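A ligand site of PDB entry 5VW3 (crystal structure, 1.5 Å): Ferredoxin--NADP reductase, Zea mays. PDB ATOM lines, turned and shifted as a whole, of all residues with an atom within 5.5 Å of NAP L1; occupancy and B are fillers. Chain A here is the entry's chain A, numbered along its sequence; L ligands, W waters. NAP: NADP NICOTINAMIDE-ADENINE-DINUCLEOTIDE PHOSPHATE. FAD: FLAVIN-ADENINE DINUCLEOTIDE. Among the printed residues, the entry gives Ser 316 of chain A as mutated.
An oxygen (O2D) of NAP L1 sits close to a nitrogen (N1) of FAD L2 (3.4 Å).
Water W6 bridges O7N of NAP L1 and O of Val 315.
Water W4 bridges O2N of NAP L1 (2.8 Å) and OG1 of Thr 53 (2.8 Å).
Water W8 lies within hydrogen-bond range of an oxygen (O1A) of NAP L1 and the backbone NH of Ala 208.
Water W9 bridges an oxygen (O1A) of NAP L1 (2.9 Å) and the guanidinium group (NH2) of Arg 238 (3.3 Å).
Water W5 lies within hydrogen-bond range of O of Ala 235 (2.9 Å), O3B of NAP L1 (3.0 Å) and N of Val 207 (3.4 Å).
Water W10 bridges the backbone carbonyl oxygen of Gly 278 (2.6 Å) and a nitrogen (N6A) of NAP L1 (3.1 Å).
The backbone carbonyl oxygen (O) of Gly 275 sits close to an oxygen (O4D) of NAP L1 (3.1 Å).
CG2 of Thr 173 touches O4B of NAP L1, 3.5 Å away.
CA of Gly 174 touches O2N of NAP L1, 3.4 Å away.
N of Gly 176 touches C6N of NAP L1, at 3.6 Å.
Gly 206 touches NAP L1.
Met 279 touches NAP L1.
C of Val 315 touches O7N of NAP L1, at 3.5 Å.
Hydrophobic or aromatic side chains that line NAP L1: Tyr 249, Leu 276 and Met 279.
Within 4 Å of NAP L1: Ser 94, Arg 114, Thr 173, Gly 174, Thr 175, Gly 176, Gly 206, Val 207, Ala 208, Ser 237, Arg 238, Lys 247, Tyr 249, Gln 251, Cys 274, Gly 275, Leu 276, Gly 278, Met 279, Glu 314, Val 315 and Ser 316.
The nearest printed residue that does not touch NAP L1 is Val 250 (4.5 Å).
O2X of NAP L1 lies within salt-bridge range of NZ of Lys 247 (2.9 Å).
O2X of NAP L1 is in salt-bridge range of NE of Arg 238 (2.9 Å).
O2N of NAP L1 lies within hydrogen-bond range of N of Thr 175 (2.9 Å).
The side-chain hydroxyl of Thr 175 lies close to an oxygen (O2N) of NAP L1 (3.3 Å).
A nitrogen (N1A) of NAP L1 is in hydrogen-bond range of the side-chain amide nitrogen of Gln 251.
The side-chain hydroxyl (OG) of Ser 316 lies close to an oxygen (O7N) of NAP L1 (3.5 Å).
An oxygen (O2X) of NAP L1 sits at hydrogen-bond distance from the side-chain hydroxyl (OG) of Ser 237.
An oxygen (O3X) of NAP L1 lies within hydrogen-bond range of the side-chain hydroxyl (OH) of Tyr 249 (2.5 Å).
NH2 of Arg 114 is in salt-bridge range of O1A of NAP L1 (2.9 Å).
An oxygen (O2) of FAD L2 lies within hydrogen-bond range of the backbone NH of Arg 114 (3.1 Å).
An oxygen (O4D) of NAP L1 is in hydrogen-bond range of the backbone NH of Leu 276 (3.2 Å).
The backbone carbonyl oxygen of Gly 278 sits at hydrogen-bond distance from a nitrogen (N6A) of NAP L1 (2.9 Å).
The backbone NH (N) of Ala 208 sits at hydrogen-bond distance from an oxygen (O3B) of NAP L1 (3.3 Å).
The backbone NH (N) of Ser 94 is in hydrogen-bond range of a nitrogen (N5) of FAD L2 (3.1 Å).
An oxygen (O3B) of NAP L1 lies close to the backbone carbonyl oxygen (O) of Val 207 (3.2 Å).
N7N of NAP L1 sits at hydrogen-bond distance from OG of Ser 94 (3.1 Å).
The side-chain carboxylate of Glu 314 sits at hydrogen-bond distance from a nitrogen (N7N) of NAP L1 (2.9 Å).
A nitrogen (N7N) of NAP L1 sits close to the side-chain sulfur (SG) of Cys 274, 3.7 Å away.
The backbone NH (N) of Gly 174 lies within hydrogen-bond range of the backbone carbonyl oxygen (O) of Gly 206, 2.9 Å away.
O of Gly 275 is in hydrogen-bond range of N of Ser 316, 3.1 Å away.
SD of Met 279 lies within hydrogen-bond range of OG1 of Thr 173 (3.3 Å).
SG of Cys 274 sits close to O of Glu 314 (3.5 Å).
The backbone NH of Leu 276 sits at hydrogen-bond distance from the side-chain hydroxyl of Thr 173 (3.0 Å).
N of Thr 173 sits at hydrogen-bond distance from O of Cys 274, 3.2 Å away.
O of Gly 176 sits close to SG of Cys 274.
N of Ser 237 lies within hydrogen-bond range of O of Ala 208 (3.4 Å).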
ATOM      1  N   PRO A  50     -16.047  -3.226 -16.331  1.00  0.00           N
ATOM      2  CA  PRO A  50     -16.092  -3.224 -14.867  1.00  0.00           C
ATOM      3  C   PRO A  50     -15.284  -4.336 -14.224  1.00  0.00           C
ATOM      4  O   PRO A  50     -14.993  -4.253 -13.019  1.00  0.00           O
ATOM      5  CB  PRO A  50     -17.577  -3.354 -14.546  1.00  0.00           C
ATOM      6  CG  PRO A  50     -18.185  -3.938 -15.753  1.00  0.00           C
ATOM      7  CD  PRO A  50     -17.379  -3.449 -16.917  1.00  0.00           C
ATOM      8  N   THR A  53     -12.769 -10.248 -17.913  1.00  0.00           N
ATOM      9  CA  THR A  53     -13.214 -11.541 -18.409  1.00  0.00           C
ATOM     10  C   THR A  53     -12.106 -12.061 -19.298  1.00  0.00           C
ATOM     11  O   THR A  53     -11.585 -11.326 -20.146  1.00  0.00           O
ATOM     12  CB  THR A  53     -14.526 -11.414 -19.188  1.00  0.00           C
ATOM     13  OG1 THR A  53     -15.534 -10.890 -18.318  1.00  0.00           O
ATOM     14  CG2 THR A  53     -14.995 -12.754 -19.691  1.00  0.00           C
ATOM     15  N   SER A  71     -20.759 -28.047 -20.277  1.00  0.00           N
ATOM     16  CA  SER A  71     -19.866 -27.393 -19.354  1.00  0.00           C
ATOM     17  C   SER A  71     -18.734 -28.338 -18.959  1.00  0.00           C
ATOM     18  O   SER A  71     -18.895 -29.558 -18.930  1.00  0.00           O
ATOM     19  CB  SER A  71     -20.600 -26.994 -18.066  1.00  0.00           C
ATOM     20  OG  SER A  71     -21.565 -25.986 -18.322  1.00  0.00           O
ATOM     21  N   SER A  94     -19.374 -22.958 -18.727  1.00  0.00           N
ATOM     22  CA  SER A  94     -19.889 -23.281 -20.049  1.00  0.00           C
ATOM     23  C   SER A  94     -18.770 -23.237 -21.078  1.00  0.00           C
ATOM     24  O   SER A  94     -18.029 -22.252 -21.173  1.00  0.00           O
ATOM     25  CB  SER A  94     -20.955 -22.271 -20.460  1.00  0.00           C
ATOM     26  OG  SER A  94     -22.169 -22.554 -19.774  1.00  0.00           O
ATOM     27  N   ARG A 114     -15.340 -14.729 -16.092  1.00  0.00           N
ATOM     28  CA  ARG A 114     -15.326 -13.439 -15.419  1.00  0.00           C
ATOM     29  C   ARG A 114     -14.663 -13.590 -14.062  1.00  0.00           C
ATOM     30  O   ARG A 114     -15.064 -14.441 -13.260  1.00  0.00           O
ATOM     31  CB  ARG A 114     -16.766 -12.954 -15.245  1.00  0.00           C
ATOM     32  CG  ARG A 114     -16.914 -11.700 -14.394  1.00  0.00           C
ATOM     33  CD  ARG A 114     -16.337 -10.478 -15.078  1.00  0.00           C
ATOM     34  NE  ARG A 114     -16.569  -9.264 -14.292  1.00  0.00           N
ATOM     35  CZ  ARG A 114     -17.600  -8.439 -14.432  1.00  0.00           C
ATOM     36  NH1 ARG A 114     -17.685  -7.374 -13.642  1.00  0.00           N
ATOM     37  NH2 ARG A 114     -18.543  -8.658 -15.364  1.00  0.00           N
ATOM     38  N   THR A 173     -26.211 -12.767 -21.428  1.00  0.00           N
ATOM     39  CA  THR A 173     -25.632 -11.682 -20.666  1.00  0.00           C
ATOM     40  C   THR A 173     -24.227 -12.071 -20.240  1.00  0.00           C
ATOM     41  O   THR A 173     -24.019 -13.149 -19.670  1.00  0.00           O
ATOM     42  CB  THR A 173     -26.482 -11.346 -19.428  1.00  0.00           C
ATOM     43  OG1 THR A 173     -26.907 -12.543 -18.778  1.00  0.00           O
ATOM     44  CG2 THR A 173     -27.685 -10.511 -19.826  1.00  0.00           C
ATOM     45  N   GLY A 174     -23.256 -11.191 -20.531  1.00  0.00           N
ATOM     46  CA  GLY A 174     -21.876 -11.412 -20.116  1.00  0.00           C
ATOM     47  C   GLY A 174     -21.340 -12.736 -20.620  1.00  0.00           C
ATOM     48  O   GLY A 174     -21.547 -13.125 -21.765  1.00  0.00           O
ATOM     49  N   THR A 175     -20.663 -13.457 -19.727  1.00  0.00           N
ATOM     50  CA  THR A 175     -20.081 -14.738 -20.063  1.00  0.00           C
ATOM     51  C   THR A 175     -21.124 -15.782 -20.432  1.00  0.00           C
ATOM     52  O   THR A 175     -20.735 -16.853 -20.917  1.00  0.00           O
ATOM     53  CB  THR A 175     -19.236 -15.288 -18.920  1.00  0.00           C
ATOM     54  OG1 THR A 175     -20.022 -15.342 -17.734  1.00  0.00           O
ATOM     55  CG2 THR A 175     -18.009 -14.415 -18.686  1.00  0.00           C
ATOM     56  N   GLY A 176     -22.412 -15.499 -20.246  1.00  0.00           N
ATOM     57  CA  GLY A 176     -23.441 -16.360 -20.819  1.00  0.00           C
ATOM     58  C   GLY A 176     -23.338 -16.496 -22.328  1.00  0.00           C
ATOM     59  O   GLY A 176     -24.006 -17.367 -22.905  1.00  0.00           O
ATOM     60  N   ALA A 178     -20.934 -17.719 -23.766  1.00  0.00           N
ATOM     61  CA  ALA A 178     -20.056 -18.856 -24.005  1.00  0.00           C
ATOM     62  C   ALA A 178     -20.637 -19.947 -24.902  1.00  0.00           C
ATOM     63  O   ALA A 178     -20.024 -20.266 -25.940  1.00  0.00           O
ATOM     64  CB  ALA A 178     -19.605 -19.448 -22.667  1.00  0.00           C
ATOM     65  N   PRO A 179     -21.775 -20.562 -24.574  1.00  0.00           N
ATOM     66  CA  PRO A 179     -22.264 -21.637 -25.450  1.00  0.00           C
ATOM     67  C   PRO A 179     -22.534 -21.145 -26.836  1.00  0.00           C
ATOM     68  O   PRO A 179     -22.412 -21.907 -27.796  1.00  0.00           O
ATOM     69  CB  PRO A 179     -23.554 -22.098 -24.764  1.00  0.00           C
ATOM     70  CG  PRO A 179     -24.007 -20.885 -23.953  1.00  0.00           C
ATOM     71  CD  PRO A 179     -22.703 -20.300 -23.462  1.00  0.00           C
ATOM     72  N   GLY A 206     -25.963  -8.893 -23.998  1.00  0.00           N
ATOM     73  CA  GLY A 206     -25.942  -7.781 -23.068  1.00  0.00           C
ATOM     74  C   GLY A 206     -24.635  -7.737 -22.291  1.00  0.00           C
ATOM     75  O   GLY A 206     -24.248  -8.736 -21.673  1.00  0.00           O
ATOM     76  N   VAL A 207     -23.939  -6.604 -22.373  1.00  0.00           N
ATOM     77  CA  VAL A 207     -22.705  -6.366 -21.630  1.00  0.00           C
ATOM     78  C   VAL A 207     -22.708  -4.917 -21.170  1.00  0.00           C
ATOM     79  O   VAL A 207     -23.553  -4.121 -21.580  1.00  0.00           O
ATOM     80  CB  VAL A 207     -21.434  -6.656 -22.451  1.00  0.00           C
ATOM     81  CG1 VAL A 207     -21.372  -8.121 -22.849  1.00  0.00           C
ATOM     82  CG2 VAL A 207     -21.365  -5.761 -23.679  1.00  0.00           C
ATOM     83  N   ALA A 208     -21.796  -4.598 -20.247  1.00  0.00           N
ATOM     84  CA  ALA A 208     -21.851  -3.305 -19.560  1.00  0.00           C
ATOM     85  C   ALA A 208     -21.594  -2.146 -20.511  1.00  0.00           C
ATOM     86  O   ALA A 208     -22.251  -1.098 -20.419  1.00  0.00           O
ATOM     87  CB  ALA A 208     -20.834  -3.287 -18.420  1.00  0.00           C
ATOM     88  N   ALA A 235     -26.938  -5.038 -26.254  1.00  0.00           N
ATOM     89  CA  ALA A 235     -27.510  -4.152 -25.244  1.00  0.00           C
ATOM     90  C   ALA A 235     -26.359  -3.752 -24.345  1.00  0.00           C
ATOM     91  O   ALA A 235     -25.885  -4.585 -23.561  1.00  0.00           O
ATOM     92  CB  ALA A 235     -28.581  -4.866 -24.443  1.00  0.00           C
ATOM     93  N   SER A 237     -25.458  -1.926 -21.290  1.00  0.00           N
ATOM     94  CA  SER A 237     -26.320  -1.473 -20.195  1.00  0.00           C
ATOM     95  C   SER A 237     -25.889  -0.119 -19.652  1.00  0.00           C
ATOM     96  O   SER A 237     -26.744   0.699 -19.261  1.00  0.00           O
ATOM     97  CB  SER A 237     -26.343  -2.512 -19.073  1.00  0.00           C
ATOM     98  OG  SER A 237     -25.035  -2.754 -18.585  1.00  0.00           O
ATOM     99  N   ARG A 238     -24.589   0.139 -19.586  1.00  0.00           N
ATOM    100  CA  ARG A 238     -24.097   1.394 -19.027  1.00  0.00           C
ATOM    101  C   ARG A 238     -23.801   2.441 -20.089  1.00  0.00           C
ATOM    102  O   ARG A 238     -23.345   3.546 -19.765  1.00  0.00           O
ATOM    103  CB  ARG A 238     -22.857   1.133 -18.169  1.00  0.00           C
ATOM    104  CG  ARG A 238     -23.126   0.054 -17.137  1.00  0.00           C
ATOM    105  CD  ARG A 238     -21.978  -0.232 -16.214  1.00  0.00           C
ATOM    106  NE  ARG A 238     -22.331  -1.330 -15.314  1.00  0.00           N
ATOM    107  CZ  ARG A 238     -21.621  -1.710 -14.257  1.00  0.00           C
ATOM    108  NH1 ARG A 238     -20.505  -1.066 -13.936  1.00  0.00           N
ATOM    109  NH2 ARG A 238     -22.029  -2.734 -13.520  1.00  0.00           N
ATOM    110  N   LYS A 247     -31.485   1.030 -17.396  1.00  0.00           N
ATOM    111  CA  LYS A 247     -30.339   0.574 -18.163  1.00  0.00           C
ATOM    112  C   LYS A 247     -30.819  -0.372 -19.260  1.00  0.00           C
ATOM    113  O   LYS A 247     -31.751  -1.142 -19.054  1.00  0.00           O
ATOM    114  CB  LYS A 247     -29.329  -0.113 -17.241  1.00  0.00           C
ATOM    115  CG  LYS A 247     -28.517   0.868 -16.424  1.00  0.00           C
ATOM    116  CD  LYS A 247     -27.160   0.294 -16.007  1.00  0.00           C
ATOM    117  CE  LYS A 247     -27.291  -0.615 -14.813  1.00  0.00           C
ATOM    118  NZ  LYS A 247     -25.999  -0.733 -14.084  1.00  0.00           N
ATOM    119  N   TYR A 249     -31.055  -3.393 -21.183  1.00  0.00           N
ATOM    120  CA  TYR A 249     -30.779  -4.794 -20.978  1.00  0.00           C
ATOM    121  C   TYR A 249     -31.254  -5.566 -22.193  1.00  0.00           C
ATOM    122  O   TYR A 249     -31.916  -5.022 -23.093  1.00  0.00           O
ATOM    123  CB  TYR A 249     -31.473  -5.275 -19.700  1.00  0.00           C
ATOM    124  CG  TYR A 249     -30.828  -4.852 -18.383  1.00  0.00           C
ATOM    125  CD1 TYR A 249     -29.481  -4.509 -18.322  1.00  0.00           C
ATOM    126  CD2 TYR A 249     -31.568  -4.834 -17.205  1.00  0.00           C
ATOM    127  CE1 TYR A 249     -28.893  -4.148 -17.127  1.00  0.00           C
ATOM    128  CE2 TYR A 249     -30.981  -4.477 -15.997  1.00  0.00           C
ATOM    129  CZ  TYR A 249     -29.643  -4.130 -15.972  1.00  0.00           C
ATOM    130  OH  TYR A 249     -29.046  -3.775 -14.786  1.00  0.00           O
ATOM    131  N   VAL A 250     -30.879  -6.839 -22.259  1.00  0.00           N
ATOM    132  CA  VAL A 250     -31.266  -7.647 -23.402  1.00  0.00           C
ATOM    133  C   VAL A 250     -32.768  -7.697 -23.558  1.00  0.00           C
ATOM    134  O   VAL A 250     -33.277  -7.752 -24.686  1.00  0.00           O
ATOM    135  CB  VAL A 250     -30.651  -9.062 -23.313  1.00  0.00           C
ATOM    136  CG1 VAL A 250     -29.181  -8.990 -23.555  1.00  0.00           C
ATOM    137  CG2 VAL A 250     -30.979  -9.722 -21.992  1.00  0.00           C
ATOM    138  N   GLN A 251     -33.521  -7.708 -22.455  1.00  0.00           N
ATOM    139  CA  GLN A 251     -34.975  -7.783 -22.588  1.00  0.00           C
ATOM    140  C   GLN A 251     -35.515  -6.574 -23.324  1.00  0.00           C
ATOM    141  O   GLN A 251     -36.535  -6.668 -24.022  1.00  0.00           O
ATOM    142  CB  GLN A 251     -35.668  -7.933 -21.230  1.00  0.00           C
ATOM    143  CG  GLN A 251     -35.207  -6.967 -20.143  1.00  0.00           C
ATOM    144  CD  GLN A 251     -34.064  -7.513 -19.318  1.00  0.00           C
ATOM    145  OE1 GLN A 251     -33.164  -8.152 -19.855  1.00  0.00           O
ATOM    146  NE2 GLN A 251     -34.090  -7.289 -18.010  1.00  0.00           N
ATOM    147  N   CYS A 274     -28.752 -17.699 -21.532  1.00  0.00           N
ATOM    148  CA  CYS A 274     -27.586 -18.101 -20.753  1.00  0.00           C
ATOM    149  C   CYS A 274     -26.954 -16.854 -20.186  1.00  0.00           C
ATOM    150  O   CYS A 274     -26.828 -15.842 -20.865  1.00  0.00           O
ATOM    151  CB  CYS A 274     -26.590 -18.854 -21.645  1.00  0.00           C
ATOM    152  SG  CYS A 274     -25.266 -19.636 -20.700  1.00  0.00           S
ATOM    153  N   GLY A 275     -26.538 -16.947 -18.926  1.00  0.00           N
ATOM    154  CA  GLY A 275     -25.938 -15.839 -18.223  1.00  0.00           C
ATOM    155  C   GLY A 275     -26.489 -15.658 -16.826  1.00  0.00           C
ATOM    156  O   GLY A 275     -26.694 -16.657 -16.115  1.00  0.00           O
ATOM    157  N   LEU A 276     -26.733 -14.412 -16.457  1.00  0.00           N
ATOM    158  CA  LEU A 276     -27.177 -14.041 -15.114  1.00  0.00           C
ATOM    159  C   LEU A 276     -28.578 -14.563 -14.867  1.00  0.00           C
ATOM    160  O   LEU A 276     -29.486 -14.294 -15.658  1.00  0.00           O
ATOM    161  CB  LEU A 276     -27.248 -12.516 -15.023  1.00  0.00           C
ATOM    162  CG  LEU A 276     -26.026 -11.647 -15.232  1.00  0.00           C
ATOM    163  CD1 LEU A 276     -26.496 -10.264 -15.644  1.00  0.00           C
ATOM    164  CD2 LEU A 276     -25.232 -11.567 -13.953  1.00  0.00           C
ATOM    165  N   GLY A 278     -30.553 -13.315 -12.863  1.00  0.00           N
ATOM    166  CA  GLY A 278     -31.378 -12.147 -12.644  1.00  0.00           C
ATOM    167  C   GLY A 278     -31.991 -11.578 -13.903  1.00  0.00           C
ATOM    168  O   GLY A 278     -32.921 -10.774 -13.798  1.00  0.00           O
ATOM    169  N   MET A 279     -31.517 -11.976 -15.084  1.00  0.00           N
ATOM    170  CA  MET A 279     -32.142 -11.434 -16.270  1.00  0.00           C
ATOM    171  C   MET A 279     -33.491 -12.089 -16.583  1.00  0.00           C
ATOM    172  O   MET A 279     -34.298 -11.502 -17.303  1.00  0.00           O
ATOM    173  CB  MET A 279     -31.230 -11.533 -17.483  1.00  0.00           C
ATOM    174  CG  MET A 279     -31.081 -12.922 -18.019  1.00  0.00           C
ATOM    175  SD  MET A 279     -30.136 -12.964 -19.539  1.00  0.00           S
ATOM    176  CE  MET A 279     -29.780 -14.678 -19.452  1.00  0.00           C
ATOM    177  N   GLU A 314     -30.220 -21.818 -19.177  1.00  0.00           N
ATOM    178  CA  GLU A 314     -29.190 -22.190 -18.223  1.00  0.00           C
ATOM    179  C   GLU A 314     -28.584 -20.898 -17.702  1.00  0.00           C
ATOM    180  O   GLU A 314     -27.818 -20.232 -18.389  1.00  0.00           O
ATOM    181  CB  GLU A 314     -28.165 -23.099 -18.894  1.00  0.00           C
ATOM    182  CG  GLU A 314     -27.579 -24.147 -17.964  1.00  0.00           C
ATOM    183  CD  GLU A 314     -26.604 -25.048 -18.693  1.00  0.00           C
ATOM    184  OE1 GLU A 314     -25.500 -24.573 -19.010  1.00  0.00           O
ATOM    185  OE2 GLU A 314     -26.935 -26.212 -18.981  1.00  0.00           O
ATOM    186  N   VAL A 315     -28.959 -20.520 -16.482  1.00  0.00           N
ATOM    187  CA  VAL A 315     -28.508 -19.278 -15.889  1.00  0.00           C
ATOM    188  C   VAL A 315     -28.089 -19.575 -14.460  1.00  0.00           C
ATOM    189  O   VAL A 315     -28.468 -20.600 -13.884  1.00  0.00           O
ATOM    190  CB  VAL A 315     -29.603 -18.186 -15.910  1.00  0.00           C
ATOM    191  CG1 VAL A 315     -29.912 -17.778 -17.350  1.00  0.00           C
ATOM    192  CG2 VAL A 315     -30.865 -18.665 -15.192  1.00  0.00           C
ATOM    193  N   SER A 316     -27.290 -18.694 -13.907  1.00  0.00           N
ATOM    194  CA  SER A 316     -26.853 -18.897 -12.530  1.00  0.00           C
ATOM    195  C   SER A 316     -26.425 -17.580 -11.932  1.00  0.00           C
ATOM    196  O   SER A 316     -26.467 -16.543 -12.591  1.00  0.00           O
ATOM    197  CB  SER A 316     -25.697 -19.885 -12.479  1.00  0.00           C
ATOM    198  OG  SER A 316     -24.593 -19.372 -13.160  1.00  0.00           O
ATOM    199  OXT SER A 316     -26.009 -17.555 -10.748  1.00  0.00           O
HETATM  200  PA  NAP L   1     -22.124  -8.891 -15.842  1.00  0.00           P
HETATM  201  O1A NAP L   1     -21.100  -7.952 -16.409  1.00  0.00           O
HETATM  202  O2A NAP L   1     -22.374  -8.940 -14.337  1.00  0.00           O
HETATM  203  O5B NAP L   1     -23.531  -8.608 -16.541  1.00  0.00           O
HETATM  204  C5B NAP L   1     -23.672  -8.780 -17.946  1.00  0.00           C
HETATM  205  C4B NAP L   1     -24.700  -7.788 -18.407  1.00  0.00           C
HETATM  206  O4B NAP L   1     -25.991  -8.126 -17.892  1.00  0.00           O
HETATM  207  C3B NAP L   1     -24.368  -6.416 -17.867  1.00  0.00           C
HETATM  208  O3B NAP L   1     -24.632  -5.455 -18.883  1.00  0.00           O
HETATM  209  C2B NAP L   1     -25.340  -6.182 -16.749  1.00  0.00           C
HETATM  210  O2B NAP L   1     -25.624  -4.798 -16.636  1.00  0.00           O
HETATM  211  C1B NAP L   1     -26.518  -6.925 -17.320  1.00  0.00           C
HETATM  212  N9A NAP L   1     -27.548  -7.207 -16.314  1.00  0.00           N
HETATM  213  C8A NAP L   1     -27.444  -7.097 -14.964  1.00  0.00           C
HETATM  214  N7A NAP L   1     -28.632  -7.410 -14.388  1.00  0.00           N
HETATM  215  C5A NAP L   1     -29.490  -7.684 -15.386  1.00  0.00           C
HETATM  216  C6A NAP L   1     -30.903  -8.071 -15.476  1.00  0.00           C
HETATM  217  N6A NAP L   1     -31.596  -8.207 -14.319  1.00  0.00           N
HETATM  218  N1A NAP L   1     -31.435  -8.262 -16.687  1.00  0.00           N
HETATM  219  C2A NAP L   1     -30.710  -8.115 -17.818  1.00  0.00           C
HETATM  220  N3A NAP L   1     -29.421  -7.756 -17.819  1.00  0.00           N
HETATM  221  C4A NAP L   1     -28.786  -7.527 -16.646  1.00  0.00           C
HETATM  222  O3  NAP L   1     -21.892 -10.345 -16.462  1.00  0.00           O
HETATM  223  PN  NAP L   1     -20.933 -11.542 -16.032  1.00  0.00           P
HETATM  224  O1N NAP L   1     -20.186 -11.203 -14.790  1.00  0.00           O
HETATM  225  O2N NAP L   1     -20.248 -12.047 -17.248  1.00  0.00           O
HETATM  226  O5D NAP L   1     -22.139 -12.488 -15.587  1.00  0.00           O
HETATM  227  C5D NAP L   1     -22.607 -13.557 -16.366  1.00  0.00           C
HETATM  228  C4D NAP L   1     -23.331 -14.447 -15.375  1.00  0.00           C
HETATM  229  O4D NAP L   1     -23.747 -15.624 -16.051  1.00  0.00           O
HETATM  230  C3D NAP L   1     -22.424 -14.868 -14.238  1.00  0.00           C
HETATM  231  O3D NAP L   1     -23.154 -14.867 -13.006  1.00  0.00           O
HETATM  232  C2D NAP L   1     -22.045 -16.284 -14.601  1.00  0.00           C
HETATM  233  O2D NAP L   1     -21.744 -17.073 -13.454  1.00  0.00           O
HETATM  234  C1D NAP L   1     -23.298 -16.730 -15.309  1.00  0.00           C
HETATM  235  N1N NAP L   1     -23.102 -17.774 -16.290  1.00  0.00           N
HETATM  236  C2N NAP L   1     -23.854 -18.866 -16.203  1.00  0.00           C
HETATM  237  C3N NAP L   1     -23.705 -19.872 -17.145  1.00  0.00           C
HETATM  238  C7N NAP L   1     -24.596 -21.066 -17.017  1.00  0.00           C
HETATM  239  O7N NAP L   1     -25.385 -21.121 -16.081  1.00  0.00           O
HETATM  240  N7N NAP L   1     -24.553 -22.029 -17.918  1.00  0.00           N
HETATM  241  C4N NAP L   1     -22.777 -19.716 -18.167  1.00  0.00           C
HETATM  242  C5N NAP L   1     -22.029 -18.559 -18.220  1.00  0.00           C
HETATM  243  C6N NAP L   1     -22.231 -17.576 -17.286  1.00  0.00           C
HETATM  244  P2B NAP L   1     -25.240  -3.937 -15.315  1.00  0.00           P
HETATM  245  O1X NAP L   1     -24.147  -4.689 -14.579  1.00  0.00           O
HETATM  246  O2X NAP L   1     -24.826  -2.635 -15.943  1.00  0.00           O
HETATM  247  O3X NAP L   1     -26.536  -3.918 -14.551  1.00  0.00           O
HETATM  248  PA  FAD L   2     -16.200 -18.743  -5.236  1.00  0.00           P
HETATM  249  O1A FAD L   2     -14.862 -18.908  -4.563  1.00  0.00           O
HETATM  250  O2A FAD L   2     -17.121 -19.906  -5.386  1.00  0.00           O
HETATM  251  O5B FAD L   2     -16.956 -17.542  -4.513  1.00  0.00           O
HETATM  252  C5B FAD L   2     -18.311 -17.273  -4.899  1.00  0.00           C
HETATM  253  C4B FAD L   2     -18.576 -15.796  -4.759  1.00  0.00           C
HETATM  254  O4B FAD L   2     -18.531 -15.458  -3.359  1.00  0.00           O
HETATM  255  C3B FAD L   2     -17.557 -14.892  -5.432  1.00  0.00           C
HETATM  256  O3B FAD L   2     -18.268 -13.815  -6.039  1.00  0.00           O
HETATM  257  C2B FAD L   2     -16.684 -14.371  -4.297  1.00  0.00           C
HETATM  258  O2B FAD L   2     -16.118 -13.099  -4.563  1.00  0.00           O
HETATM  259  C1B FAD L   2     -17.712 -14.313  -3.216  1.00  0.00           C
HETATM  260  N9A FAD L   2     -17.173 -14.395  -1.854  1.00  0.00           N
HETATM  261  C8A FAD L   2     -16.267 -15.290  -1.405  1.00  0.00           C
HETATM  262  N7A FAD L   2     -16.034 -15.089  -0.078  1.00  0.00           N
HETATM  263  C5A FAD L   2     -16.810 -14.064   0.285  1.00  0.00           C
HETATM  264  C6A FAD L   2     -17.071 -13.318   1.525  1.00  0.00           C
HETATM  265  N6A FAD L   2     -16.437 -13.652   2.653  1.00  0.00           N
HETATM  266  N1A FAD L   2     -17.952 -12.300   1.486  1.00  0.00           N
HETATM  267  C2A FAD L   2     -18.613 -11.941   0.380  1.00  0.00           C
HETATM  268  N3A FAD L   2     -18.422 -12.574  -0.792  1.00  0.00           N
HETATM  269  C4A FAD L   2     -17.553 -13.604  -0.861  1.00  0.00           C
HETATM  270  N1  FAD L   2     -18.934 -18.369 -14.797  1.00  0.00           N
HETATM  271  C2  FAD L   2     -18.191 -17.821 -15.761  1.00  0.00           C
HETATM  272  O2  FAD L   2     -17.465 -16.838 -15.489  1.00  0.00           O
HETATM  273  N3  FAD L   2     -18.218 -18.307 -17.012  1.00  0.00           N
HETATM  274  C4  FAD L   2     -18.968 -19.333 -17.385  1.00  0.00           C
HETATM  275  O4  FAD L   2     -18.948 -19.754 -18.572  1.00  0.00           O
HETATM  276  C4X FAD L   2     -19.802 -19.993 -16.388  1.00  0.00           C
HETATM  277  N5  FAD L   2     -20.584 -21.049 -16.675  1.00  0.00           N
HETATM  278  C5X FAD L   2     -21.284 -21.672 -15.695  1.00  0.00           C
HETATM  279  C6  FAD L   2     -22.071 -22.773 -16.002  1.00  0.00           C
HETATM  280  C7  FAD L   2     -22.849 -23.376 -15.040  1.00  0.00           C
HETATM  281  C7M FAD L   2     -23.694 -24.554 -15.392  1.00  0.00           C
HETATM  282  C8  FAD L   2     -22.854 -22.815 -13.680  1.00  0.00           C
HETATM  283  C8M FAD L   2     -23.702 -23.420 -12.587  1.00  0.00           C
HETATM  284  C9  FAD L   2     -22.069 -21.732 -13.363  1.00  0.00           C
HETATM  285  C9A FAD L   2     -21.291 -21.128 -14.325  1.00  0.00           C
HETATM  286  N10 FAD L   2     -20.445 -20.043 -14.036  1.00  0.00           N
HETATM  287  C10 FAD L   2     -19.745 -19.416 -15.052  1.00  0.00           C
HETATM  288  C1' FAD L   2     -20.139 -19.599 -12.653  1.00  0.00           C
HETATM  289  C2' FAD L   2     -18.961 -20.384 -12.109  1.00  0.00           C
HETATM  290  O2' FAD L   2     -19.285 -21.751 -11.955  1.00  0.00           O
HETATM  291  C3' FAD L   2     -18.521 -19.908 -10.729  1.00  0.00           C
HETATM  292  O3' FAD L   2     -19.630 -19.940  -9.822  1.00  0.00           O
HETATM  293  C4' FAD L   2     -17.933 -18.520 -10.763  1.00  0.00           C
HETATM  294  O4' FAD L   2     -16.786 -18.513 -11.625  1.00  0.00           O
HETATM  295  C5' FAD L   2     -17.439 -18.104  -9.399  1.00  0.00           C
HETATM  296  O5' FAD L   2     -16.635 -19.147  -8.862  1.00  0.00           O
HETATM  297  P   FAD L   2     -15.331 -18.821  -7.989  1.00  0.00           P
HETATM  298  O1P FAD L   2     -14.520 -17.782  -8.678  1.00  0.00           O
HETATM  299  O2P FAD L   2     -14.702 -20.115  -7.578  1.00  0.00           O
HETATM  300  O3P FAD L   2     -15.941 -18.063  -6.677  1.00  0.00           O
HETATM  301  O   HOH W   1     -22.553 -10.595 -12.078  1.00  0.00           O
HETATM  302  O   HOH W   2     -28.694  -7.299 -20.560  1.00  0.00           O
HETATM  303  O   HOH W   3     -26.055 -14.393 -11.216  1.00  0.00           O
HETATM  304  O   HOH W   4     -18.311 -10.598 -18.573  1.00  0.00           O
HETATM  305  O   HOH W   5     -26.783  -5.466 -20.908  1.00  0.00           O
HETATM  306  O   HOH W   6     -26.888 -22.889 -14.664  1.00  0.00           O
HETATM  307  O   HOH W   7     -28.315  -9.602 -11.864  1.00  0.00           O
HETATM  308  O   HOH W   8     -20.597  -6.999 -18.952  1.00  0.00           O
HETATM  309  O   HOH W   9     -21.411  -5.181 -15.640  1.00  0.00           O
HETATM  310  O   HOH W  10     -34.656  -8.915 -14.498  1.00  0.00           O
HETATM  311  O   HOH W  11     -20.902 -16.214 -10.435  1.00  0.00           O
